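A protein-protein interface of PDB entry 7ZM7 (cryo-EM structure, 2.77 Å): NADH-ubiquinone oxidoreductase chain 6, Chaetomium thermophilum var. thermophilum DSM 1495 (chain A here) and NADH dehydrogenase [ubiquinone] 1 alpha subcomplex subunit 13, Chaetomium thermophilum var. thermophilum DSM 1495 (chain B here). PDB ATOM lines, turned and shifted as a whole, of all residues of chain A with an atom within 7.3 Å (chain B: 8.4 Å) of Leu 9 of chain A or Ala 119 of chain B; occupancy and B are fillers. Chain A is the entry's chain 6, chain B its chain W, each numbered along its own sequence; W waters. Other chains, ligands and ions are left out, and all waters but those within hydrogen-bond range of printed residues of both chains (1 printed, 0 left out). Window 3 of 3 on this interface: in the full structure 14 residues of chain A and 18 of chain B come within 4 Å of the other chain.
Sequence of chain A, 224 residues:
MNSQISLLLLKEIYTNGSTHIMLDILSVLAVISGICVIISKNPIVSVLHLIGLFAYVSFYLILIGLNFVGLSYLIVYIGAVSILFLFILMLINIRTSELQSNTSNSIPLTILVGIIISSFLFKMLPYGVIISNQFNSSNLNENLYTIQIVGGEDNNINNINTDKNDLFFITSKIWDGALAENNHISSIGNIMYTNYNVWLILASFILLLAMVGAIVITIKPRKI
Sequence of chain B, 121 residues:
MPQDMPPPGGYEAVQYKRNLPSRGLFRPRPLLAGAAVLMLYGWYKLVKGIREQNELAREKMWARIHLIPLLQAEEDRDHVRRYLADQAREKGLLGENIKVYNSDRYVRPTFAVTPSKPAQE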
ATOM      1  N   ILE A   5      -3.130 -18.584 -24.092  1.00  0.00           N
ATOM      2  CA  ILE A   5      -4.360 -18.577 -23.251  1.00  0.00           C
ATOM      3  C   ILE A   5      -5.517 -18.019 -24.089  1.00  0.00           C
ATOM      4  O   ILE A   5      -5.350 -16.946 -24.698  1.00  0.00           O
ATOM      5  CB  ILE A   5      -4.110 -17.778 -21.955  1.00  0.00           C
ATOM      6  CG1 ILE A   5      -3.633 -16.350 -22.235  1.00  0.00           C
ATOM      7  CG2 ILE A   5      -3.125 -18.514 -21.065  1.00  0.00           C
ATOM      8  CD1 ILE A   5      -3.387 -15.529 -20.992  1.00  0.00           C
ATOM      9  N   SER A   6      -6.635 -18.748 -24.151  1.00  0.00           N
ATOM     10  CA  SER A   6      -7.786 -18.320 -24.989  1.00  0.00           C
ATOM     11  C   SER A   6      -8.449 -17.074 -24.409  1.00  0.00           C
ATOM     12  O   SER A   6      -8.823 -16.190 -25.191  1.00  0.00           O
ATOM     13  CB  SER A   6      -8.746 -19.432 -25.205  1.00  0.00           C
ATOM     14  OG  SER A   6      -8.151 -20.464 -25.976  1.00  0.00           O
ATOM     15  N   LEU A   7      -8.595 -17.021 -23.085  1.00  0.00           N
ATOM     16  CA  LEU A   7      -9.178 -15.825 -22.430  1.00  0.00           C
ATOM     17  C   LEU A   7      -8.113 -14.735 -22.415  1.00  0.00           C
ATOM     18  O   LEU A   7      -6.992 -15.034 -21.996  1.00  0.00           O
ATOM     19  CB  LEU A   7      -9.612 -16.193 -21.011  1.00  0.00           C
ATOM     20  CG  LEU A   7     -10.764 -17.184 -20.892  1.00  0.00           C
ATOM     21  CD1 LEU A   7     -10.998 -17.539 -19.432  1.00  0.00           C
ATOM     22  CD2 LEU A   7     -12.031 -16.613 -21.512  1.00  0.00           C
ATOM     23  N   LEU A   8      -8.462 -13.522 -22.845  1.00  0.00           N
ATOM     24  CA  LEU A   8      -7.496 -12.399 -22.940  1.00  0.00           C
ATOM     25  C   LEU A   8      -8.011 -11.182 -22.167  1.00  0.00           C
ATOM     26  O   LEU A   8      -9.139 -10.763 -22.427  1.00  0.00           O
ATOM     27  CB  LEU A   8      -7.272 -12.083 -24.420  1.00  0.00           C
ATOM     28  CG  LEU A   8      -6.318 -13.019 -25.156  1.00  0.00           C
ATOM     29  CD1 LEU A   8      -5.928 -12.424 -26.497  1.00  0.00           C
ATOM     30  CD2 LEU A   8      -5.075 -13.283 -24.322  1.00  0.00           C
ATOM     31  N   LEU A   9      -7.298 -10.651 -21.247  1.00  0.00           N
ATOM     32  CA  LEU A   9      -7.747  -9.495 -20.433  1.00  0.00           C
ATOM     33  C   LEU A   9      -6.847  -8.301 -20.748  1.00  0.00           C
ATOM     34  O   LEU A   9      -5.622  -8.443 -20.605  1.00  0.00           O
ATOM     35  CB  LEU A   9      -7.626  -9.878 -18.956  1.00  0.00           C
ATOM     36  CG  LEU A   9      -8.297  -8.931 -17.963  1.00  0.00           C
ATOM     37  CD1 LEU A   9      -9.785  -8.815 -18.252  1.00  0.00           C
ATOM     38  CD2 LEU A   9      -8.073  -9.409 -16.538  1.00  0.00           C
ATOM     39  N   LEU A  10      -7.381  -7.210 -21.156  1.00  0.00           N
ATOM     40  CA  LEU A  10      -6.645  -5.989 -21.438  1.00  0.00           C
ATOM     41  C   LEU A  10      -7.431  -4.773 -20.973  1.00  0.00           C
ATOM     42  O   LEU A  10      -8.657  -4.791 -20.872  1.00  0.00           O
ATOM     43  CB  LEU A  10      -6.297  -5.846 -22.918  1.00  0.00           C
ATOM     44  CG  LEU A  10      -7.340  -5.509 -23.968  1.00  0.00           C
ATOM     45  CD1 LEU A  10      -6.638  -5.051 -25.220  1.00  0.00           C
ATOM     46  CD2 LEU A  10      -8.127  -6.738 -24.270  1.00  0.00           C
ATOM     47  N   LYS A  11      -6.739  -3.648 -20.756  1.00  0.00           N
ATOM     48  CA  LYS A  11      -7.395  -2.400 -20.255  1.00  0.00           C
ATOM     49  C   LYS A  11      -8.266  -1.741 -21.338  1.00  0.00           C
ATOM     50  O   LYS A  11      -8.137  -2.131 -22.512  1.00  0.00           O
ATOM     51  CB  LYS A  11      -6.308  -1.427 -19.785  1.00  0.00           C
ATOM     52  CG  LYS A  11      -6.770  -0.253 -18.932  1.00  0.00           C
ATOM     53  CD  LYS A  11      -5.802   0.907 -18.965  1.00  0.00           C
ATOM     54  CE  LYS A  11      -6.350   2.154 -18.305  1.00  0.00           C
ATOM     55  NZ  LYS A  11      -5.388   3.279 -18.372  1.00  0.00           N
ATOM     56  N   PHE A 168     -15.431 -11.221 -11.255  1.00  0.00           N
ATOM     57  CA  PHE A 168     -15.661 -10.037 -12.057  1.00  0.00           C
ATOM     58  C   PHE A 168     -17.033 -10.118 -12.698  1.00  0.00           C
ATOM     59  O   PHE A 168     -17.437 -11.163 -13.204  1.00  0.00           O
ATOM     60  CB  PHE A 168     -14.595  -9.895 -13.144  1.00  0.00           C
ATOM     61  CG  PHE A 168     -13.349  -9.217 -12.687  1.00  0.00           C
ATOM     62  CD1 PHE A 168     -13.231  -7.845 -12.760  1.00  0.00           C
ATOM     63  CD2 PHE A 168     -12.272  -9.953 -12.237  1.00  0.00           C
ATOM     64  CE1 PHE A 168     -12.087  -7.220 -12.355  1.00  0.00           C
ATOM     65  CE2 PHE A 168     -11.126  -9.334 -11.835  1.00  0.00           C
ATOM     66  CZ  PHE A 168     -11.031  -7.963 -11.894  1.00  0.00           C
ATOM     67  N   ALA B 112     -17.731 -13.786 -15.189  1.00  0.00           N
ATOM     68  CA  ALA B 112     -16.838 -14.443 -16.128  1.00  0.00           C
ATOM     69  C   ALA B 112     -15.584 -14.900 -15.403  1.00  0.00           C
ATOM     70  O   ALA B 112     -15.174 -14.318 -14.400  1.00  0.00           O
ATOM     71  CB  ALA B 112     -16.452 -13.525 -17.294  1.00  0.00           C
ATOM     72  N   VAL B 113     -15.004 -15.961 -15.904  1.00  0.00           N
ATOM     73  CA  VAL B 113     -13.673 -16.368 -15.484  1.00  0.00           C
ATOM     74  C   VAL B 113     -12.660 -15.530 -16.238  1.00  0.00           C
ATOM     75  O   VAL B 113     -12.721 -15.404 -17.463  1.00  0.00           O
ATOM     76  CB  VAL B 113     -13.476 -17.871 -15.725  1.00  0.00           C
ATOM     77  CG1 VAL B 113     -12.063 -18.270 -15.526  1.00  0.00           C
ATOM     78  CG2 VAL B 113     -14.337 -18.616 -14.773  1.00  0.00           C
ATOM     79  N   THR B 114     -11.745 -14.925 -15.502  1.00  0.00           N
ATOM     80  CA  THR B 114     -10.773 -14.025 -16.079  1.00  0.00           C
ATOM     81  C   THR B 114      -9.388 -14.511 -15.704  1.00  0.00           C
ATOM     82  O   THR B 114      -9.229 -15.255 -14.730  1.00  0.00           O
ATOM     83  CB  THR B 114     -10.952 -12.572 -15.604  1.00  0.00           C
ATOM     84  OG1 THR B 114     -11.204 -12.550 -14.204  1.00  0.00           O
ATOM     85  CG2 THR B 114     -12.083 -11.894 -16.321  1.00  0.00           C
ATOM     86  N   PRO B 115      -8.370 -14.124 -16.469  1.00  0.00           N
ATOM     87  CA  PRO B 115      -6.997 -14.310 -16.007  1.00  0.00           C
ATOM     88  C   PRO B 115      -6.733 -13.516 -14.743  1.00  0.00           C
ATOM     89  O   PRO B 115      -7.404 -12.532 -14.431  1.00  0.00           O
ATOM     90  CB  PRO B 115      -6.148 -13.794 -17.164  1.00  0.00           C
ATOM     91  CG  PRO B 115      -7.060 -13.683 -18.308  1.00  0.00           C
ATOM     92  CD  PRO B 115      -8.436 -13.558 -17.817  1.00  0.00           C
ATOM     93  N   SER B 116      -5.743 -13.976 -13.996  1.00  0.00           N
ATOM     94  CA  SER B 116      -5.336 -13.252 -12.806  1.00  0.00           C
ATOM     95  C   SER B 116      -4.578 -11.975 -13.146  1.00  0.00           C
ATOM     96  O   SER B 116      -4.445 -11.100 -12.288  1.00  0.00           O
ATOM     97  CB  SER B 116      -4.520 -14.177 -11.911  1.00  0.00           C
ATOM     98  OG  SER B 116      -3.578 -14.901 -12.676  1.00  0.00           O
ATOM     99  N   LYS B 117      -4.089 -11.832 -14.377  1.00  0.00           N
ATOM    100  CA  LYS B 117      -3.368 -10.628 -14.761  1.00  0.00           C
ATOM    101  C   LYS B 117      -3.770 -10.141 -16.145  1.00  0.00           C
ATOM    102  O   LYS B 117      -4.112 -10.938 -17.020  1.00  0.00           O
ATOM    103  CB  LYS B 117      -1.852 -10.866 -14.744  1.00  0.00           C
ATOM    104  CG  LYS B 117      -1.276 -11.144 -13.362  1.00  0.00           C
ATOM    105  CD  LYS B 117      -1.427  -9.938 -12.452  1.00  0.00           C
ATOM    106  CE  LYS B 117      -0.427  -8.854 -12.805  1.00  0.00           C
ATOM    107  NZ  LYS B 117       0.970  -9.281 -12.516  1.00  0.00           N
ATOM    108  N   PRO B 118      -3.723  -8.836 -16.371  1.00  0.00           N
ATOM    109  CA  PRO B 118      -3.922  -8.313 -17.726  1.00  0.00           C
ATOM    110  C   PRO B 118      -2.685  -8.449 -18.591  1.00  0.00           C
ATOM    111  O   PRO B 118      -1.669  -8.997 -18.157  1.00  0.00           O
ATOM    112  CB  PRO B 118      -4.254  -6.837 -17.486  1.00  0.00           C
ATOM    113  CG  PRO B 118      -4.535  -6.721 -16.044  1.00  0.00           C
ATOM    114  CD  PRO B 118      -3.706  -7.755 -15.381  1.00  0.00           C
ATOM    115  N   ALA B 119      -2.756  -7.953 -19.820  1.00  0.00           N
ATOM    116  CA  ALA B 119      -1.572  -7.876 -20.657  1.00  0.00           C
ATOM    117  C   ALA B 119      -0.556  -6.919 -20.045  1.00  0.00           C
ATOM    118  O   ALA B 119      -0.899  -6.015 -19.278  1.00  0.00           O
ATOM    119  CB  ALA B 119      -1.936  -7.416 -22.065  1.00  0.00           C
ATOM    120  N   GLN B 120       0.715  -7.134 -20.383  1.00  0.00           N
ATOM    121  CA  GLN B 120       1.783  -6.333 -19.795  1.00  0.00           C
ATOM    122  C   GLN B 120       1.637  -4.862 -20.160  1.00  0.00           C
ATOM    123  O   GLN B 120       1.856  -3.978 -19.325  1.00  0.00           O
ATOM    124  CB  GLN B 120       3.144  -6.869 -20.235  1.00  0.00           C
ATOM    125  CG  GLN B 120       3.667  -7.997 -19.364  1.00  0.00           C
ATOM    126  CD  GLN B 120       2.828  -9.253 -19.474  1.00  0.00           C
ATOM    127  OE1 GLN B 120       2.282  -9.736 -18.484  1.00  0.00           O
ATOM    128  NE2 GLN B 120       2.719  -9.786 -20.683  1.00  0.00           N
ATOM    129  N   GLU B 121       1.268  -4.583 -21.407  1.00  0.00           N
ATOM    130  CA  GLU B 121       1.117  -3.216 -21.903  1.00  0.00           C
ATOM    131  C   GLU B 121       2.408  -2.421 -21.747  1.00  0.00           C
ATOM    132  O   GLU B 121       3.498  -2.941 -21.986  1.00  0.00           O
ATOM    133  CB  GLU B 121      -0.029  -2.499 -21.183  1.00  0.00           C
HETATM  134  O   HOH W   1     -14.074 -13.125 -12.550  1.00  0.00           O
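Printed residues of chain B within 4 Å of Leu 7 of chain A: Val 113 (3.4 Å) and Pro 115 (3.9 Å).
Printed residues of chain A within 4 Å of Ala 112 of chain B: Phe 168.
Printed residues of chain A within 4 Å of Val 113 of chain B: Leu 7 (3.4 Å).
The nearest residue of chain B that does not touch Leu 9 of chain A is Lys 117 of chain B (4.1 Å).
Val 113 of chain B touches Leu 7 of chain A (O to CD1, 3.4 Å).
Pro 115 of chain B touches Leu 7 of chain A (CG to O, 3.9 Å).
CD2 of Leu 9 of chain A touches O of Pro 115 of chain B (3.8 Å).
CA of Pro 118 of chain B touches O of Leu 9 of chain A (3.3 Å).
Phe 168 of chain A touches Thr 114 of chain B.
N of Ala 112 of chain B is in hydrogen-bond range of O of Phe 168 of chain A (3.3 Å).
N of Ala 119 of chain B is in hydrogen-bond range of O of Leu 9 of chain A (3.0 Å).
Water W1 lies within hydrogen-bond range of O of Ala 112 of chain B (2.5 Å), N of Phe 168 of chain A (2.7 Å) and OG1 of Thr 114 of chain B (3.4 Å).
Hydrophobic or aromatic side chains of chain A within 4 Å of the printed part of chain B: Leu 7, Leu 9 and Phe 168.
Along chain A the printed residues that touch a printed residue of chain B span positions 7 to 168.
Printed residues of chain B that touch a printed residue of chain A: Ala 112, Val 113, Thr 114, Pro 115, Pro 118 and Ala 119.
Among the printed residues, no Asp or Glu carboxylate lies within 4 Å of a Lys or Arg side-chain nitrogen of the other chain.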
